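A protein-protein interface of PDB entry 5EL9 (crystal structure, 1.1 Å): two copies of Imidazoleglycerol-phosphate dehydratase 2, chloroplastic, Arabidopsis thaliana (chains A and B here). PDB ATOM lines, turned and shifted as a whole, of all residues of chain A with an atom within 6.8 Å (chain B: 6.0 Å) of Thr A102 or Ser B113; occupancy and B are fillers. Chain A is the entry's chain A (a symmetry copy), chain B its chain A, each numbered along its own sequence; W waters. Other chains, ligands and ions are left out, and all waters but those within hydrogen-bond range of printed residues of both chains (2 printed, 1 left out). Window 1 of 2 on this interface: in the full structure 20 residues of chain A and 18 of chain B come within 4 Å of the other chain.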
ATOM      1  N   ASP A 100     -31.388 -32.633   7.817  1.00  0.00           N
ATOM      2  CA  ASP A 100     -31.870 -31.301   7.496  1.00  0.00           C
ATOM      3  C   ASP A 100     -30.809 -30.585   6.692  1.00  0.00           C
ATOM      4  O   ASP A 100     -29.713 -30.324   7.186  1.00  0.00           O
ATOM      5  CB  ASP A 100     -32.149 -30.568   8.812  1.00  0.00           C
ATOM      6  CG  ASP A 100     -32.642 -29.192   8.627  1.00  0.00           C
ATOM      7  OD1 ASP A 100     -33.390 -28.923   7.677  1.00  0.00           O
ATOM      8  OD2 ASP A 100     -32.279 -28.355   9.481  1.00  0.00           O
ATOM      9  N   PHE A 101     -31.122 -30.245   5.446  1.00  0.00           N
ATOM     10  CA  PHE A 101     -30.145 -29.561   4.624  1.00  0.00           C
ATOM     11  C   PHE A 101     -30.846 -28.762   3.535  1.00  0.00           C
ATOM     12  O   PHE A 101     -31.819 -29.224   2.941  1.00  0.00           O
ATOM     13  CB  PHE A 101     -29.144 -30.550   3.993  1.00  0.00           C
ATOM     14  CG  PHE A 101     -27.849 -29.885   3.619  1.00  0.00           C
ATOM     15  CD1 PHE A 101     -26.976 -29.464   4.619  1.00  0.00           C
ATOM     16  CD2 PHE A 101     -27.534 -29.563   2.305  1.00  0.00           C
ATOM     17  CE1 PHE A 101     -25.814 -28.793   4.329  1.00  0.00           C
ATOM     18  CE2 PHE A 101     -26.373 -28.879   2.011  1.00  0.00           C
ATOM     19  CZ  PHE A 101     -25.514 -28.493   3.011  1.00  0.00           C
ATOM     20  N   THR A 102     -30.306 -27.574   3.259  1.00  0.00           N
ATOM     21  CA  THR A 102     -30.721 -26.745   2.149  1.00  0.00           C
ATOM     22  C   THR A 102     -29.567 -26.590   1.178  1.00  0.00           C
ATOM     23  O   THR A 102     -28.502 -26.135   1.579  1.00  0.00           O
ATOM     24  CB  THR A 102     -31.214 -25.366   2.630  1.00  0.00           C
ATOM     25  OG1 THR A 102     -32.338 -25.544   3.508  1.00  0.00           O
ATOM     26  CG2 THR A 102     -31.658 -24.510   1.506  1.00  0.00           C
ATOM     27  N   ALA A 103     -29.798 -26.975  -0.075  1.00  0.00           N
ATOM     28  CA  ALA A 103     -28.784 -26.929  -1.125  1.00  0.00           C
ATOM     29  C   ALA A 103     -29.231 -26.017  -2.256  1.00  0.00           C
ATOM     30  O   ALA A 103     -30.381 -26.108  -2.706  1.00  0.00           O
ATOM     31  CB  ALA A 103     -28.481 -28.299  -1.698  1.00  0.00           C
ATOM     32  N   PRO A 104     -28.319 -25.192  -2.774  1.00  0.00           N
ATOM     33  CA  PRO A 104     -28.611 -24.465  -3.990  1.00  0.00           C
ATOM     34  C   PRO A 104     -28.142 -25.211  -5.209  1.00  0.00           C
ATOM     35  O   PRO A 104     -27.280 -26.089  -5.131  1.00  0.00           O
ATOM     36  CB  PRO A 104     -27.797 -23.196  -3.847  1.00  0.00           C
ATOM     37  CG  PRO A 104     -26.820 -23.426  -2.791  1.00  0.00           C
ATOM     38  CD  PRO A 104     -27.052 -24.751  -2.175  1.00  0.00           C
ATOM     39  N   LEU A 109     -32.919 -23.060  -4.859  1.00  0.00           N
ATOM     40  CA  LEU A 109     -32.593 -23.285  -3.452  1.00  0.00           C
ATOM     41  C   LEU A 109     -33.687 -24.140  -2.847  1.00  0.00           C
ATOM     42  O   LEU A 109     -34.843 -23.722  -2.827  1.00  0.00           O
ATOM     43  CB  LEU A 109     -32.480 -21.947  -2.709  1.00  0.00           C
ATOM     44  CG  LEU A 109     -31.989 -22.064  -1.271  1.00  0.00           C
ATOM     45  CD1 LEU A 109     -30.521 -22.458  -1.220  1.00  0.00           C
ATOM     46  CD2 LEU A 109     -32.177 -20.753  -0.541  1.00  0.00           C
ATOM     47  N   ILE A 110     -33.317 -25.341  -2.383  1.00  0.00           N
ATOM     48  CA  ILE A 110     -34.294 -26.325  -1.935  1.00  0.00           C
ATOM     49  C   ILE A 110     -33.925 -26.823  -0.542  1.00  0.00           C
ATOM     50  O   ILE A 110     -32.791 -27.247  -0.313  1.00  0.00           O
ATOM     51  CB  ILE A 110     -34.393 -27.520  -2.902  1.00  0.00           C
ATOM     52  CG1 ILE A 110     -34.594 -27.068  -4.346  1.00  0.00           C
ATOM     53  CG2 ILE A 110     -35.495 -28.454  -2.422  1.00  0.00           C
ATOM     54  CD1 ILE A 110     -35.898 -26.390  -4.678  1.00  0.00           C
ATOM     55  N   HIS A 111     -34.892 -26.715   0.385  1.00  0.00           N
ATOM     56  CA  HIS A 111     -34.730 -27.230   1.732  1.00  0.00           C
ATOM     57  C   HIS A 111     -35.367 -28.603   1.840  1.00  0.00           C
ATOM     58  O   HIS A 111     -36.549 -28.781   1.530  1.00  0.00           O
ATOM     59  CB  HIS A 111     -35.404 -26.274   2.685  1.00  0.00           C
ATOM     60  CG  HIS A 111     -35.401 -26.748   4.102  1.00  0.00           C
ATOM     61  ND1 HIS A 111     -36.461 -26.553   4.941  1.00  0.00           N
ATOM     62  CD2 HIS A 111     -34.491 -27.438   4.828  1.00  0.00           C
ATOM     63  CE1 HIS A 111     -36.194 -27.054   6.130  1.00  0.00           C
ATOM     64  NE2 HIS A 111     -34.988 -27.584   6.092  1.00  0.00           N
ATOM     65  N   VAL A 112     -34.592 -29.569   2.331  1.00  0.00           N
ATOM     66  CA  VAL A 112     -35.100 -30.899   2.651  1.00  0.00           C
ATOM     67  C   VAL A 112     -34.881 -31.204   4.132  1.00  0.00           C
ATOM     68  O   VAL A 112     -33.777 -31.076   4.636  1.00  0.00           O
ATOM     69  CB  VAL A 112     -34.463 -31.976   1.789  1.00  0.00           C
ATOM     70  CG1 VAL A 112     -34.905 -33.358   2.255  1.00  0.00           C
ATOM     71  CG2 VAL A 112     -34.800 -31.733   0.330  1.00  0.00           C
ATOM     72  N   ARG A 159     -39.062 -28.224   0.343  1.00  0.00           N
ATOM     73  CA  ARG A 159     -39.539 -26.837   0.240  1.00  0.00           C
ATOM     74  C   ARG A 159     -38.719 -26.088  -0.797  1.00  0.00           C
ATOM     75  O   ARG A 159     -37.492 -25.967  -0.675  1.00  0.00           O
ATOM     76  CB  ARG A 159     -39.454 -26.115   1.582  1.00  0.00           C
ATOM     77  CG  ARG A 159     -40.234 -26.688   2.749  1.00  0.00           C
ATOM     78  CD  ARG A 159     -40.302 -25.686   3.928  1.00  0.00           C
ATOM     79  NE  ARG A 159     -38.997 -25.137   4.360  1.00  0.00           N
ATOM     80  CZ  ARG A 159     -38.696 -23.837   4.572  1.00  0.00           C
ATOM     81  NH1 ARG A 159     -39.577 -22.846   4.410  1.00  0.00           N
ATOM     82  NH2 ARG A 159     -37.476 -23.500   4.979  1.00  0.00           N
ATOM     83  N   LEU A 161     -37.421 -22.829  -1.999  1.00  0.00           N
ATOM     84  CA  LEU A 161     -37.151 -21.477  -1.483  1.00  0.00           C
ATOM     85  C   LEU A 161     -36.868 -20.492  -2.608  1.00  0.00           C
ATOM     86  O   LEU A 161     -37.117 -19.306  -2.430  1.00  0.00           O
ATOM     87  CB  LEU A 161     -36.005 -21.514  -0.474  1.00  0.00           C
ATOM     88  CG  LEU A 161     -36.193 -22.493   0.685  1.00  0.00           C
ATOM     89  CD1 LEU A 161     -34.985 -22.396   1.607  1.00  0.00           C
ATOM     90  CD2 LEU A 161     -37.491 -22.215   1.443  1.00  0.00           C
ATOM     91  N   ALA A 172     -31.195 -29.571  -7.441  1.00  0.00           N
ATOM     92  CA  ALA A 172     -30.970 -29.067  -6.075  1.00  0.00           C
ATOM     93  C   ALA A 172     -31.755 -29.895  -5.062  1.00  0.00           C
ATOM     94  O   ALA A 172     -31.293 -30.160  -3.948  1.00  0.00           O
ATOM     95  CB  ALA A 172     -31.335 -27.603  -5.974  1.00  0.00           C
ATOM     96  N   ALA A 176     -30.018 -31.785  -1.940  1.00  0.00           N
ATOM     97  CA  ALA A 176     -30.434 -31.520  -0.566  1.00  0.00           C
ATOM     98  C   ALA A 176     -30.925 -32.803   0.105  1.00  0.00           C
ATOM     99  O   ALA A 176     -30.593 -33.095   1.260  1.00  0.00           O
ATOM    100  CB  ALA A 176     -31.524 -30.467  -0.520  1.00  0.00           C
ATOM    101  N   ARG A 179     -27.985 -35.097   0.996  1.00  0.00           N
ATOM    102  CA  ARG A 179     -27.241 -34.653   2.186  1.00  0.00           C
ATOM    103  C   ARG A 179     -28.045 -34.843   3.453  1.00  0.00           C
ATOM    104  O   ARG A 179     -27.514 -35.245   4.487  1.00  0.00           O
ATOM    105  CB  ARG A 179     -26.810 -33.212   2.040  1.00  0.00           C
ATOM    106  CG  ARG A 179     -25.733 -33.085   0.988  1.00  0.00           C
ATOM    107  CD  ARG A 179     -24.342 -33.283   1.522  1.00  0.00           C
ATOM    108  NE  ARG A 179     -23.403 -33.396   0.416  1.00  0.00           N
ATOM    109  CZ  ARG A 179     -22.183 -32.871   0.352  1.00  0.00           C
ATOM    110  NH1 ARG A 179     -21.467 -33.084  -0.763  1.00  0.00           N
ATOM    111  NH2 ARG A 179     -21.678 -32.141   1.339  1.00  0.00           N
ATOM    112  N   PHE B  98     -20.815 -27.849   0.085  1.00  0.00           N
ATOM    113  CA  PHE B  98     -22.036 -27.166   0.467  1.00  0.00           C
ATOM    114  C   PHE B  98     -21.964 -26.733   1.926  1.00  0.00           C
ATOM    115  O   PHE B  98     -21.504 -27.472   2.794  1.00  0.00           O
ATOM    116  CB  PHE B  98     -23.246 -28.091   0.288  1.00  0.00           C
ATOM    117  CG  PHE B  98     -23.529 -28.463  -1.138  1.00  0.00           C
ATOM    118  CD1 PHE B  98     -22.970 -29.581  -1.730  1.00  0.00           C
ATOM    119  CD2 PHE B  98     -24.373 -27.673  -1.900  1.00  0.00           C
ATOM    120  CE1 PHE B  98     -23.236 -29.886  -3.048  1.00  0.00           C
ATOM    121  CE2 PHE B  98     -24.654 -27.989  -3.211  1.00  0.00           C
ATOM    122  CZ  PHE B  98     -24.072 -29.084  -3.786  1.00  0.00           C
ATOM    123  N   GLY B  99     -22.518 -25.560   2.201  1.00  0.00           N
ATOM    124  CA  GLY B  99     -22.697 -25.059   3.559  1.00  0.00           C
ATOM    125  C   GLY B  99     -24.077 -24.471   3.725  1.00  0.00           C
ATOM    126  O   GLY B  99     -24.637 -23.925   2.773  1.00  0.00           O
ATOM    127  N   ASP B 100     -24.610 -24.591   4.930  1.00  0.00           N
ATOM    128  CA  ASP B 100     -25.981 -24.193   5.197  1.00  0.00           C
ATOM    129  C   ASP B 100     -26.111 -23.871   6.668  1.00  0.00           C
ATOM    130  O   ASP B 100     -25.950 -24.745   7.521  1.00  0.00           O
ATOM    131  CB  ASP B 100     -26.897 -25.356   4.806  1.00  0.00           C
ATOM    132  CG  ASP B 100     -28.327 -25.082   5.035  1.00  0.00           C
ATOM    133  OD1 ASP B 100     -28.777 -23.942   4.858  1.00  0.00           O
ATOM    134  OD2 ASP B 100     -29.027 -26.056   5.388  1.00  0.00           O
ATOM    135  N   PHE B 101     -26.416 -22.618   6.989  1.00  0.00           N
ATOM    136  CA  PHE B 101     -26.550 -22.248   8.382  1.00  0.00           C
ATOM    137  C   PHE B 101     -27.447 -21.026   8.515  1.00  0.00           C
ATOM    138  O   PHE B 101     -27.363 -20.093   7.717  1.00  0.00           O
ATOM    139  CB  PHE B 101     -25.178 -21.969   9.029  1.00  0.00           C
ATOM    140  CG  PHE B 101     -25.210 -22.130  10.523  1.00  0.00           C
ATOM    141  CD1 PHE B 101     -25.340 -23.402  11.077  1.00  0.00           C
ATOM    142  CD2 PHE B 101     -25.236 -21.042  11.385  1.00  0.00           C
ATOM    143  CE1 PHE B 101     -25.442 -23.593  12.432  1.00  0.00           C
ATOM    144  CE2 PHE B 101     -25.349 -21.230  12.747  1.00  0.00           C
ATOM    145  CZ  PHE B 101     -25.453 -22.493  13.274  1.00  0.00           C
ATOM    146  N   HIS B 111     -30.626 -16.741   7.098  1.00  0.00           N
ATOM    147  CA  HIS B 111     -30.235 -18.023   6.542  1.00  0.00           C
ATOM    148  C   HIS B 111     -29.263 -17.814   5.397  1.00  0.00           C
ATOM    149  O   HIS B 111     -29.552 -17.086   4.443  1.00  0.00           O
ATOM    150  CB  HIS B 111     -31.478 -18.718   6.043  1.00  0.00           C
ATOM    151  CG  HIS B 111     -31.196 -20.009   5.347  1.00  0.00           C
ATOM    152  ND1 HIS B 111     -31.895 -20.415   4.246  1.00  0.00           N
ATOM    153  CD2 HIS B 111     -30.274 -20.977   5.564  1.00  0.00           C
ATOM    154  CE1 HIS B 111     -31.456 -21.589   3.840  1.00  0.00           C
ATOM    155  NE2 HIS B 111     -30.478 -21.963   4.640  1.00  0.00           N
ATOM    156  N   VAL B 112     -28.122 -18.498   5.467  1.00  0.00           N
ATOM    157  CA  VAL B 112     -27.157 -18.535   4.372  1.00  0.00           C
ATOM    158  C   VAL B 112     -26.947 -19.975   3.905  1.00  0.00           C
ATOM    159  O   VAL B 112     -26.664 -20.852   4.705  1.00  0.00           O
ATOM    160  CB  VAL B 112     -25.830 -17.905   4.759  1.00  0.00           C
ATOM    161  CG1 VAL B 112     -24.807 -18.100   3.646  1.00  0.00           C
ATOM    162  CG2 VAL B 112     -26.035 -16.440   5.093  1.00  0.00           C
ATOM    163  N   SER B 113     -27.088 -20.178   2.605  1.00  0.00           N
ATOM    164  CA  SER B 113     -26.790 -21.450   1.959  1.00  0.00           C
ATOM    165  C   SER B 113     -25.846 -21.177   0.816  1.00  0.00           C
ATOM    166  O   SER B 113     -26.085 -20.274   0.032  1.00  0.00           O
ATOM    167  CB  SER B 113     -28.093 -22.068   1.441  1.00  0.00           C
ATOM    168  OG  SER B 113     -27.925 -23.359   0.930  1.00  0.00           O
ATOM    169  N   LEU B 114     -24.795 -21.991   0.686  1.00  0.00           N
ATOM    170  CA  LEU B 114     -23.844 -21.780  -0.377  1.00  0.00           C
ATOM    171  C   LEU B 114     -23.299 -23.084  -0.926  1.00  0.00           C
ATOM    172  O   LEU B 114     -23.287 -24.115  -0.237  1.00  0.00           O
ATOM    173  CB  LEU B 114     -22.746 -20.797   0.043  1.00  0.00           C
ATOM    174  CG  LEU B 114     -21.796 -21.239   1.143  1.00  0.00           C
ATOM    175  CD1 LEU B 114     -20.613 -22.004   0.586  1.00  0.00           C
ATOM    176  CD2 LEU B 114     -21.309 -20.033   1.943  1.00  0.00           C
ATOM    177  N   ASP B 115     -22.843 -23.003  -2.167  1.00  0.00           N
ATOM    178  CA  ASP B 115     -22.268 -24.119  -2.897  1.00  0.00           C
ATOM    179  C   ASP B 115     -21.005 -23.605  -3.543  1.00  0.00           C
ATOM    180  O   ASP B 115     -21.061 -22.703  -4.372  1.00  0.00           O
ATOM    181  CB  ASP B 115     -23.276 -24.640  -3.941  1.00  0.00           C
ATOM    182  CG  ASP B 115     -22.725 -25.679  -4.872  1.00  0.00           C
ATOM    183  OD1 ASP B 115     -21.625 -26.176  -4.569  1.00  0.00           O
ATOM    184  OD2 ASP B 115     -23.398 -26.001  -5.887  1.00  0.00           O
ATOM    185  N   THR B 155     -21.931 -20.130  -5.432  1.00  0.00           N
ATOM    186  CA  THR B 155     -23.373 -19.942  -5.418  1.00  0.00           C
ATOM    187  C   THR B 155     -23.772 -19.616  -3.981  1.00  0.00           C
ATOM    188  O   THR B 155     -23.507 -20.412  -3.095  1.00  0.00           O
ATOM    189  CB  THR B 155     -24.071 -21.228  -5.835  1.00  0.00           C
ATOM    190  OG1 THR B 155     -23.600 -21.688  -7.101  1.00  0.00           O
ATOM    191  CG2 THR B 155     -25.577 -21.068  -5.847  1.00  0.00           C
ATOM    192  N   LEU B 156     -24.386 -18.464  -3.752  1.00  0.00           N
ATOM    193  CA  LEU B 156     -24.666 -17.973  -2.411  1.00  0.00           C
ATOM    194  C   LEU B 156     -26.092 -17.437  -2.333  1.00  0.00           C
ATOM    195  O   LEU B 156     -26.457 -16.597  -3.149  1.00  0.00           O
ATOM    196  CB  LEU B 156     -23.659 -16.853  -2.066  1.00  0.00           C
ATOM    197  CG  LEU B 156     -23.862 -16.126  -0.752  1.00  0.00           C
ATOM    198  CD1 LEU B 156     -23.763 -17.049   0.443  1.00  0.00           C
ATOM    199  CD2 LEU B 156     -22.804 -15.041  -0.626  1.00  0.00           C
ATOM    200  N   HIS B 157     -26.843 -17.922  -1.354  1.00  0.00           N
ATOM    201  CA  HIS B 157     -28.178 -17.406  -1.047  1.00  0.00           C
ATOM    202  C   HIS B 157     -28.185 -16.875   0.362  1.00  0.00           C
ATOM    203  O   HIS B 157     -27.779 -17.567   1.303  1.00  0.00           O
ATOM    204  CB  HIS B 157     -29.244 -18.500  -1.188  1.00  0.00           C
ATOM    205  CG  HIS B 157     -29.480 -18.903  -2.602  1.00  0.00           C
ATOM    206  ND1 HIS B 157     -30.622 -18.532  -3.280  1.00  0.00           N
ATOM    207  CD2 HIS B 157     -28.729 -19.625  -3.461  1.00  0.00           C
ATOM    208  CE1 HIS B 157     -30.552 -19.027  -4.498  1.00  0.00           C
ATOM    209  NE2 HIS B 157     -29.414 -19.685  -4.639  1.00  0.00           N
ATOM    210  N   ILE B 158     -28.729 -15.670   0.516  1.00  0.00           N
ATOM    211  CA  ILE B 158     -28.873 -14.967   1.793  1.00  0.00           C
ATOM    212  C   ILE B 158     -30.338 -14.580   1.943  1.00  0.00           C
ATOM    213  O   ILE B 158     -30.848 -13.835   1.116  1.00  0.00           O
ATOM    214  CB  ILE B 158     -27.948 -13.739   1.851  1.00  0.00           C
ATOM    215  CG1 ILE B 158     -26.478 -14.129   1.686  1.00  0.00           C
ATOM    216  CG2 ILE B 158     -28.213 -12.953   3.125  1.00  0.00           C
ATOM    217  CD1 ILE B 158     -25.495 -12.986   1.636  1.00  0.00           C
ATOM    218  N   ALA B 180     -21.548 -21.118   7.387  1.00  0.00           N
ATOM    219  CA  ALA B 180     -21.809 -21.867   6.159  1.00  0.00           C
ATOM    220  C   ALA B 180     -20.528 -22.063   5.341  1.00  0.00           C
ATOM    221  O   ALA B 180     -20.278 -23.139   4.809  1.00  0.00           O
ATOM    222  CB  ALA B 180     -22.876 -21.161   5.329  1.00  0.00           C
HETATM  223  O   HOH W   1     -25.557 -27.555  -6.692  1.00  0.00           O
HETATM  224  O   HOH W   2     -31.595 -26.245   6.042  1.00  0.00           O
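Water W2 lies within hydrogen-bond range of OD2 of Asp B100 (2.7 Å) and OG1 of Thr A102 (2.7 Å). Water W1 lies within hydrogen-bond range of the backbone carbonyl oxygen (O) of Pro A104 and the side-chain carboxylate (OD2) of Asp B115.
Phe A101 touches Asp B100, but with the chains exchanged Asp A100 does not touch Phe B101 (8.4 Å). Of the 14 pairs that touch across the chains among the printed residues, none has its exchanged pair printed and touching as well.
Of the printed residues of chain B, Arg A179 touches Phe B98. Printed residues of chain A within 4 Å of Asp B100: Phe A101 (3.6 Å) and Thr A102 (2.9 Å). Of the printed residues of chain A, His B111 touches Thr A102. Of the printed residues of chain A, Leu B114 touches Pro A104 (3.999 Å). Printed residues of chain A within 4 Å of Thr B155: Pro A104 (3.7 Å).
The side-chain hydroxyl (OG) of Ser B113 lies within hydrogen-bond range of the backbone carbonyl oxygen (O) of Thr A102 (2.9 Å). The side-chain carboxylate of Asp B100 lies within hydrogen-bond range of the backbone NH of Thr A102.
Among the printed residues, merely in contact across the chains: Leu A109 with Ser B113 (3.5 Å), Pro A104 with Ser B113 (3.5 Å), Phe A101 with Phe B98 (3.6 Å), Phe A101 with Asp B100 (3.6 Å), Pro A104 with Thr B155 (3.7 Å), Pro A104 with His B157 (3.7 Å), Thr A102 with His B111 (3.7 Å), Leu A109 with His B157 (3.8 Å), Pro A104 with Phe B98 (3.8 Å), Pro A104 with Asp B115 (3.9 Å), Arg A179 with Phe B98 (3.9 Å) and Pro A104 with Leu B114 (3.999 Å).
The backbone NH (N) of Leu B114 sits at hydrogen-bond distance from the backbone carbonyl oxygen (O) of Gly B99, 2.8 Å away. The backbone carbonyl oxygen (O) of Leu A109 lies within hydrogen-bond range of the backbone NH (N) of Leu A161 (2.9 Å). The backbone carbonyl oxygen (O) of Phe A101 lies within hydrogen-bond range of the backbone NH (N) of Val A112, at 2.9 Å. N of Asp B115 is in hydrogen-bond range of O of Thr B155. NE2 of His B111 is in hydrogen-bond range of OD1 of Asp B100 (2.6 Å). The backbone carbonyl oxygen (O) of Ser B113 is in hydrogen-bond range of the backbone NH (N) of His B157 (2.8 Å).
Hydrophobic or aromatic side chains of chain B that line the printed part of chain A: Phe B98, His B111 and His B157.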
